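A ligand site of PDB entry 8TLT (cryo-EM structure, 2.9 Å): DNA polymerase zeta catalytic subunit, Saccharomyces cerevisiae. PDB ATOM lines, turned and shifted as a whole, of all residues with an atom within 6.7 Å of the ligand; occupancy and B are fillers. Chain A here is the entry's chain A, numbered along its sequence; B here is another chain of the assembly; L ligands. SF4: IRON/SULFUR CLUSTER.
The side-chain sulfur (SG) of Cys 1502 is bound to an iron atom (FE3) of the ligand (2.3 Å). A sulfur (S2) of the ligand lies close to the backbone NH (N) of Phe 1510 (3.7 Å). An iron atom (FE1) of the ligand is bound by the side-chain sulfur (SG) of Cys 1507 (2.3 Å). An iron atom (FE2) of the ligand is bound by the side-chain sulfur of Cys 1483 (2.3 Å). FE4 of the ligand is bound by SG of Cys 1480 (2.3 Å).
SG of Cys 1480 sits close to O of Leu 1476 (3.6 Å). SG of Cys 1502 lies close to N of Ser 1504 (3.4 Å). The side-chain sulfur of Cys 1507 sits close to the backbone NH of Val 1509 (3.5 Å). The side-chain sulfur (SG) of Cys 1502 lies close to the backbone carbonyl oxygen (O) of His 889 (3.7 Å). NH1 of Arg 886 sits at hydrogen-bond distance from O of Asp 1506 (3.2 Å). NE of Arg 1513 lies close to SG of Cys 1480, 3.7 Å away. O of Cys 1502 is in hydrogen-bond range of NH2 of Arg 1513 (3.2 Å).
Arg 886 touches the ligand (CG to S4, 3.9 Å). Val 1509 touches the ligand (CB to FE1, 3.9 Å). NH2 of Arg 1513 touches S2 of the ligand, at 3.9 Å. Hydrophobic or aromatic side chains within 4 Å of the ligand: Val 1509 and Phe 1510. Of the 27 residues printed, 8 come within 4 Å of the ligand. Along chain A the residues within 4 Å of the ligand span positions 886 to 1513.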
ATOM      1  N   ARG A 886     -28.753 -35.521   5.972  1.00  0.00           N
ATOM      2  CA  ARG A 886     -28.172 -34.377   6.646  1.00  0.00           C
ATOM      3  C   ARG A 886     -27.556 -34.821   7.963  1.00  0.00           C
ATOM      4  O   ARG A 886     -28.248 -35.391   8.811  1.00  0.00           O
ATOM      5  CB  ARG A 886     -29.223 -33.290   6.884  1.00  0.00           C
ATOM      6  CG  ARG A 886     -28.714 -32.083   7.622  1.00  0.00           C
ATOM      7  CD  ARG A 886     -27.628 -31.385   6.832  1.00  0.00           C
ATOM      8  NE  ARG A 886     -28.159 -30.636   5.700  1.00  0.00           N
ATOM      9  CZ  ARG A 886     -27.417 -30.111   4.743  1.00  0.00           C
ATOM     10  NH1 ARG A 886     -26.093 -30.222   4.750  1.00  0.00           N
ATOM     11  NH2 ARG A 886     -27.999 -29.451   3.746  1.00  0.00           N
ATOM     12  N   LEU A 887     -26.268 -34.563   8.139  1.00  0.00           N
ATOM     13  CA  LEU A 887     -25.551 -34.969   9.333  1.00  0.00           C
ATOM     14  C   LEU A 887     -25.141 -33.737  10.123  1.00  0.00           C
ATOM     15  O   LEU A 887     -24.488 -32.840   9.570  1.00  0.00           O
ATOM     16  CB  LEU A 887     -24.317 -35.797   8.973  1.00  0.00           C
ATOM     17  CG  LEU A 887     -24.503 -37.016   8.071  1.00  0.00           C
ATOM     18  CD1 LEU A 887     -23.162 -37.429   7.474  1.00  0.00           C
ATOM     19  CD2 LEU A 887     -25.109 -38.162   8.846  1.00  0.00           C
ATOM     20  N   PRO A 888     -25.509 -33.634  11.401  1.00  0.00           N
ATOM     21  CA  PRO A 888     -24.960 -32.563  12.235  1.00  0.00           C
ATOM     22  C   PRO A 888     -23.450 -32.690  12.359  1.00  0.00           C
ATOM     23  O   PRO A 888     -22.904 -33.796  12.435  1.00  0.00           O
ATOM     24  CB  PRO A 888     -25.649 -32.787  13.594  1.00  0.00           C
ATOM     25  CG  PRO A 888     -26.867 -33.573  13.279  1.00  0.00           C
ATOM     26  CD  PRO A 888     -26.540 -34.427  12.102  1.00  0.00           C
ATOM     27  N   HIS A 889     -22.780 -31.549  12.366  1.00  0.00           N
ATOM     28  CA  HIS A 889     -21.327 -31.486  12.488  1.00  0.00           C
ATOM     29  C   HIS A 889     -20.965 -30.808  13.798  1.00  0.00           C
ATOM     30  O   HIS A 889     -21.441 -29.704  14.089  1.00  0.00           O
ATOM     31  CB  HIS A 889     -20.705 -30.738  11.311  1.00  0.00           C
ATOM     32  CG  HIS A 889     -19.227 -30.549  11.421  1.00  0.00           C
ATOM     33  ND1 HIS A 889     -18.643 -29.303  11.549  1.00  0.00           N
ATOM     34  CD2 HIS A 889     -18.207 -31.436  11.428  1.00  0.00           C
ATOM     35  CE1 HIS A 889     -17.338 -29.442  11.635  1.00  0.00           C
ATOM     36  NE2 HIS A 889     -17.046 -30.724  11.561  1.00  0.00           N
ATOM     37  N   PHE A 890     -20.117 -31.465  14.593  1.00  0.00           N
ATOM     38  CA  PHE A 890     -19.649 -30.921  15.865  1.00  0.00           C
ATOM     39  C   PHE A 890     -18.156 -30.662  15.782  1.00  0.00           C
ATOM     40  O   PHE A 890     -17.409 -31.415  15.150  1.00  0.00           O
ATOM     41  CB  PHE A 890     -19.938 -31.887  17.016  1.00  0.00           C
ATOM     42  CG  PHE A 890     -21.383 -32.307  17.104  1.00  0.00           C
ATOM     43  CD1 PHE A 890     -22.404 -31.390  16.943  1.00  0.00           C
ATOM     44  CD2 PHE A 890     -21.709 -33.624  17.357  1.00  0.00           C
ATOM     45  CE1 PHE A 890     -23.725 -31.779  17.024  1.00  0.00           C
ATOM     46  CE2 PHE A 890     -23.028 -34.017  17.447  1.00  0.00           C
ATOM     47  CZ  PHE A 890     -24.037 -33.092  17.277  1.00  0.00           C
ATOM     48  N   LEU A1476     -36.939 -23.231  14.080  1.00  0.00           N
ATOM     49  CA  LEU A1476     -35.569 -23.644  13.780  1.00  0.00           C
ATOM     50  C   LEU A1476     -35.029 -24.577  14.846  1.00  0.00           C
ATOM     51  O   LEU A1476     -34.359 -25.566  14.531  1.00  0.00           O
ATOM     52  CB  LEU A1476     -34.675 -22.404  13.649  1.00  0.00           C
ATOM     53  CG  LEU A1476     -34.840 -21.607  12.352  1.00  0.00           C
ATOM     54  CD1 LEU A1476     -33.850 -20.466  12.315  1.00  0.00           C
ATOM     55  CD2 LEU A1476     -34.671 -22.508  11.147  1.00  0.00           C
ATOM     56  N   VAL A1479     -36.522 -28.006  14.373  1.00  0.00           N
ATOM     57  CA  VAL A1479     -35.886 -28.685  13.247  1.00  0.00           C
ATOM     58  C   VAL A1479     -34.531 -29.233  13.647  1.00  0.00           C
ATOM     59  O   VAL A1479     -34.185 -30.381  13.335  1.00  0.00           O
ATOM     60  CB  VAL A1479     -35.780 -27.728  12.045  1.00  0.00           C
ATOM     61  CG1 VAL A1479     -34.779 -28.243  11.034  1.00  0.00           C
ATOM     62  CG2 VAL A1479     -37.139 -27.530  11.392  1.00  0.00           C
ATOM     63  N   CYS A1480     -33.732 -28.421  14.338  1.00  0.00           N
ATOM     64  CA  CYS A1480     -32.398 -28.858  14.749  1.00  0.00           C
ATOM     65  C   CYS A1480     -32.469 -30.019  15.747  1.00  0.00           C
ATOM     66  O   CYS A1480     -31.643 -30.930  15.699  1.00  0.00           O
ATOM     67  CB  CYS A1480     -31.616 -27.693  15.330  1.00  0.00           C
ATOM     68  SG  CYS A1480     -30.905 -26.592  14.091  1.00  0.00           S
ATOM     69  N   ARG A1481     -33.439 -29.983  16.662  1.00  0.00           N
ATOM     70  CA  ARG A1481     -33.605 -31.066  17.624  1.00  0.00           C
ATOM     71  C   ARG A1481     -33.989 -32.357  16.914  1.00  0.00           C
ATOM     72  O   ARG A1481     -33.438 -33.431  17.217  1.00  0.00           O
ATOM     73  CB  ARG A1481     -34.654 -30.676  18.652  1.00  0.00           C
ATOM     74  CG  ARG A1481     -34.793 -31.623  19.819  1.00  0.00           C
ATOM     75  CD  ARG A1481     -35.924 -31.163  20.738  1.00  0.00           C
ATOM     76  NE  ARG A1481     -35.876 -29.720  20.952  1.00  0.00           N
ATOM     77  CZ  ARG A1481     -36.886 -28.893  20.702  1.00  0.00           C
ATOM     78  NH1 ARG A1481     -38.040 -29.338  20.224  1.00  0.00           N
ATOM     79  NH2 ARG A1481     -36.728 -27.594  20.929  1.00  0.00           N
ATOM     80  N   THR A1482     -34.914 -32.283  15.957  1.00  0.00           N
ATOM     81  CA  THR A1482     -35.277 -33.468  15.193  1.00  0.00           C
ATOM     82  C   THR A1482     -34.088 -34.013  14.403  1.00  0.00           C
ATOM     83  O   THR A1482     -33.910 -35.229  14.290  1.00  0.00           O
ATOM     84  CB  THR A1482     -36.444 -33.161  14.255  1.00  0.00           C
ATOM     85  N   CYS A1483     -33.267 -33.114  13.844  1.00  0.00           N
ATOM     86  CA  CYS A1483     -32.075 -33.545  13.118  1.00  0.00           C
ATOM     87  C   CYS A1483     -31.080 -34.234  14.041  1.00  0.00           C
ATOM     88  O   CYS A1483     -30.537 -35.295  13.713  1.00  0.00           O
ATOM     89  CB  CYS A1483     -31.426 -32.353  12.414  1.00  0.00           C
ATOM     90  SG  CYS A1483     -29.974 -32.767  11.427  1.00  0.00           S
ATOM     91  N   SER A1484     -30.826 -33.648  15.213  1.00  0.00           N
ATOM     92  CA  SER A1484     -29.875 -34.217  16.166  1.00  0.00           C
ATOM     93  C   SER A1484     -30.382 -35.488  16.819  1.00  0.00           C
ATOM     94  O   SER A1484     -29.579 -36.204  17.438  1.00  0.00           O
ATOM     95  CB  SER A1484     -29.531 -33.181  17.245  1.00  0.00           C
ATOM     96  N   ALA A1499     -28.017 -30.542  20.062  1.00  0.00           N
ATOM     97  CA  ALA A1499     -28.475 -29.930  18.819  1.00  0.00           C
ATOM     98  C   ALA A1499     -27.928 -28.512  18.675  1.00  0.00           C
ATOM     99  O   ALA A1499     -27.569 -28.089  17.569  1.00  0.00           O
ATOM    100  CB  ALA A1499     -30.001 -29.921  18.776  1.00  0.00           C
ATOM    101  N   CYS A1502     -24.192 -28.040  17.371  1.00  0.00           N
ATOM    102  CA  CYS A1502     -23.856 -28.240  15.964  1.00  0.00           C
ATOM    103  C   CYS A1502     -23.329 -26.957  15.346  1.00  0.00           C
ATOM    104  O   CYS A1502     -23.817 -25.857  15.638  1.00  0.00           O
ATOM    105  CB  CYS A1502     -25.078 -28.736  15.193  1.00  0.00           C
ATOM    106  SG  CYS A1502     -24.891 -28.693  13.390  1.00  0.00           S
ATOM    107  N   ASN A1503     -22.324 -27.085  14.483  1.00  0.00           N
ATOM    108  CA  ASN A1503     -21.788 -25.949  13.728  1.00  0.00           C
ATOM    109  C   ASN A1503     -21.527 -26.349  12.284  1.00  0.00           C
ATOM    110  O   ASN A1503     -20.488 -26.018  11.698  1.00  0.00           O
ATOM    111  CB  ASN A1503     -20.520 -25.404  14.379  1.00  0.00           C
ATOM    112  CG  ASN A1503     -19.388 -26.410  14.400  1.00  0.00           C
ATOM    113  OD1 ASN A1503     -19.605 -27.612  14.509  1.00  0.00           O
ATOM    114  ND2 ASN A1503     -18.161 -25.919  14.282  1.00  0.00           N
ATOM    115  N   SER A1504     -22.471 -27.066  11.674  1.00  0.00           N
ATOM    116  CA  SER A1504     -22.312 -27.507  10.296  1.00  0.00           C
ATOM    117  C   SER A1504     -22.455 -26.330   9.343  1.00  0.00           C
ATOM    118  O   SER A1504     -23.526 -25.706   9.288  1.00  0.00           O
ATOM    119  CB  SER A1504     -23.328 -28.591   9.973  1.00  0.00           C
ATOM    120  OG  SER A1504     -23.674 -28.579   8.606  1.00  0.00           O
ATOM    121  N   ASP A1506     -22.401 -26.495   6.098  1.00  0.00           N
ATOM    122  CA  ASP A1506     -23.024 -26.914   4.845  1.00  0.00           C
ATOM    123  C   ASP A1506     -24.539 -26.899   4.905  1.00  0.00           C
ATOM    124  O   ASP A1506     -25.195 -27.224   3.914  1.00  0.00           O
ATOM    125  CB  ASP A1506     -22.543 -28.316   4.457  1.00  0.00           C
ATOM    126  CG  ASP A1506     -21.054 -28.492   4.651  1.00  0.00           C
ATOM    127  OD1 ASP A1506     -20.276 -27.994   3.809  1.00  0.00           O
ATOM    128  OD2 ASP A1506     -20.653 -29.128   5.646  1.00  0.00           O
ATOM    129  N   CYS A1507     -25.117 -26.500   6.034  1.00  0.00           N
ATOM    130  CA  CYS A1507     -26.566 -26.512   6.226  1.00  0.00           C
ATOM    131  C   CYS A1507     -27.092 -25.086   6.308  1.00  0.00           C
ATOM    132  O   CYS A1507     -26.588 -24.299   7.106  1.00  0.00           O
ATOM    133  CB  CYS A1507     -26.922 -27.276   7.507  1.00  0.00           C
ATOM    134  SG  CYS A1507     -28.695 -27.463   7.784  1.00  0.00           S
ATOM    135  N   PRO A1508     -28.084 -24.725   5.488  1.00  0.00           N
ATOM    136  CA  PRO A1508     -28.681 -23.386   5.598  1.00  0.00           C
ATOM    137  C   PRO A1508     -29.403 -23.154   6.908  1.00  0.00           C
ATOM    138  O   PRO A1508     -29.556 -21.999   7.324  1.00  0.00           O
ATOM    139  CB  PRO A1508     -29.638 -23.322   4.407  1.00  0.00           C
ATOM    140  CG  PRO A1508     -29.952 -24.741   4.105  1.00  0.00           C
ATOM    141  CD  PRO A1508     -28.722 -25.529   4.425  1.00  0.00           C
ATOM    142  N   VAL A1509     -29.876 -24.215   7.576  1.00  0.00           N
ATOM    143  CA  VAL A1509     -30.557 -24.062   8.854  1.00  0.00           C
ATOM    144  C   VAL A1509     -29.603 -23.520   9.905  1.00  0.00           C
ATOM    145  O   VAL A1509     -30.005 -22.751  10.787  1.00  0.00           O
ATOM    146  CB  VAL A1509     -31.199 -25.392   9.290  1.00  0.00           C
ATOM    147  CG1 VAL A1509     -31.958 -25.220  10.590  1.00  0.00           C
ATOM    148  CG2 VAL A1509     -32.127 -25.902   8.204  1.00  0.00           C
ATOM    149  N   PHE A1510     -28.326 -23.919   9.852  1.00  0.00           N
ATOM    150  CA  PHE A1510     -27.340 -23.381  10.784  1.00  0.00           C
ATOM    151  C   PHE A1510     -27.184 -21.875  10.606  1.00  0.00           C
ATOM    152  O   PHE A1510     -27.151 -21.123  11.593  1.00  0.00           O
ATOM    153  CB  PHE A1510     -26.003 -24.096  10.582  1.00  0.00           C
ATOM    154  CG  PHE A1510     -24.873 -23.502  11.359  1.00  0.00           C
ATOM    155  CD1 PHE A1510     -24.833 -23.599  12.739  1.00  0.00           C
ATOM    156  CD2 PHE A1510     -23.841 -22.844  10.716  1.00  0.00           C
ATOM    157  CE1 PHE A1510     -23.786 -23.063  13.447  1.00  0.00           C
ATOM    158  CE2 PHE A1510     -22.794 -22.307  11.424  1.00  0.00           C
ATOM    159  CZ  PHE A1510     -22.761 -22.409  12.793  1.00  0.00           C
ATOM    160  N   TYR A1511     -27.092 -21.411   9.364  1.00  0.00           N
ATOM    161  CA  TYR A1511     -26.994 -19.975   9.107  1.00  0.00           C
ATOM    162  C   TYR A1511     -28.255 -19.249   9.558  1.00  0.00           C
ATOM    163  O   TYR A1511     -28.167 -18.170  10.153  1.00  0.00           O
ATOM    164  CB  TYR A1511     -26.749 -19.728   7.613  1.00  0.00           C
ATOM    165  CG  TYR A1511     -25.382 -20.164   7.134  1.00  0.00           C
ATOM    166  CD1 TYR A1511     -24.295 -19.297   7.185  1.00  0.00           C
ATOM    167  CD2 TYR A1511     -25.174 -21.439   6.630  1.00  0.00           C
ATOM    168  CE1 TYR A1511     -23.054 -19.687   6.750  1.00  0.00           C
ATOM    169  CE2 TYR A1511     -23.923 -21.838   6.201  1.00  0.00           C
ATOM    170  CZ  TYR A1511     -22.874 -20.962   6.263  1.00  0.00           C
ATOM    171  OH  TYR A1511     -21.625 -21.356   5.825  1.00  0.00           O
ATOM    172  N   ARG A1513     -30.321 -20.160  11.953  1.00  0.00           N
ATOM    173  CA  ARG A1513     -30.334 -20.151  13.415  1.00  0.00           C
ATOM    174  C   ARG A1513     -29.366 -19.115  13.970  1.00  0.00           C
ATOM    175  O   ARG A1513     -29.695 -18.410  14.931  1.00  0.00           O
ATOM    176  CB  ARG A1513     -30.012 -21.540  13.946  1.00  0.00           C
ATOM    177  CG  ARG A1513     -29.315 -21.558  15.293  1.00  0.00           C
ATOM    178  CD  ARG A1513     -29.410 -22.920  15.943  1.00  0.00           C
ATOM    179  NE  ARG A1513     -28.640 -23.922  15.223  1.00  0.00           N
ATOM    180  CZ  ARG A1513     -27.382 -24.240  15.480  1.00  0.00           C
ATOM    181  NH1 ARG A1513     -26.700 -23.630  16.432  1.00  0.00           N
ATOM    182  NH2 ARG A1513     -26.787 -25.187  14.761  1.00  0.00           N
ATOM    183  N   GLY B 135     -34.767 -25.245   4.083  1.00  0.00           N
ATOM    184  CA  GLY B 135     -33.545 -26.031   4.126  1.00  0.00           C
ATOM    185  C   GLY B 135     -33.630 -27.166   5.116  1.00  0.00           C
ATOM    186  O   GLY B 135     -32.628 -27.850   5.368  1.00  0.00           O
ATOM    187  N   ALA B 136     -34.810 -27.380   5.680  1.00  0.00           N
ATOM    188  CA  ALA B 136     -34.985 -28.463   6.622  1.00  0.00           C
ATOM    189  C   ALA B 136     -34.798 -29.806   5.922  1.00  0.00           C
ATOM    190  O   ALA B 136     -35.292 -29.994   4.800  1.00  0.00           O
ATOM    191  CB  ALA B 136     -36.371 -28.400   7.264  1.00  0.00           C
ATOM    192  N   PRO B 137     -34.092 -30.742   6.532  1.00  0.00           N
ATOM    193  CA  PRO B 137     -33.910 -32.056   5.902  1.00  0.00           C
ATOM    194  C   PRO B 137     -35.163 -32.905   5.978  1.00  0.00           C
ATOM    195  O   PRO B 137     -36.184 -32.467   6.531  1.00  0.00           O
ATOM    196  CB  PRO B 137     -32.767 -32.684   6.726  1.00  0.00           C
ATOM    197  CG  PRO B 137     -32.284 -31.592   7.662  1.00  0.00           C
ATOM    198  CD  PRO B 137     -33.418 -30.652   7.833  1.00  0.00           C
ATOM    199  N   LEU B 139     -36.913 -34.937   7.900  1.00  0.00           N
ATOM    200  CA  LEU B 139     -36.895 -35.340   9.297  1.00  0.00           C
ATOM    201  C   LEU B 139     -37.517 -36.714   9.496  1.00  0.00           C
ATOM    202  O   LEU B 139     -37.157 -37.430  10.438  1.00  0.00           O
ATOM    203  CB  LEU B 139     -37.626 -34.296  10.142  1.00  0.00           C
ATOM    204  CG  LEU B 139     -37.063 -32.871  10.055  1.00  0.00           C
ATOM    205  CD1 LEU B 139     -37.764 -31.943  11.030  1.00  0.00           C
ATOM    206  CD2 LEU B 139     -35.565 -32.872  10.307  1.00  0.00           C
HETATM  207 FE1  SF4 L   1     -28.582 -28.195   9.927  1.00  0.00          FE
HETATM  208 FE2  SF4 L   1     -29.185 -30.651  11.549  1.00  0.00          FE
HETATM  209 FE3  SF4 L   1     -26.875 -28.879  12.317  1.00  0.00          FE
HETATM  210 FE4  SF4 L   1     -29.702 -27.934  12.709  1.00  0.00          FE
HETATM  211  S1  SF4 L   1     -28.607 -29.613  13.315  1.00  0.00           S
HETATM  212  S2  SF4 L   1     -28.010 -27.165  11.690  1.00  0.00           S
HETATM  213  S3  SF4 L   1     -30.294 -28.947  10.935  1.00  0.00           S
HETATM  214  S4  SF4 L   1     -27.471 -29.904  10.549  1.00  0.00           S
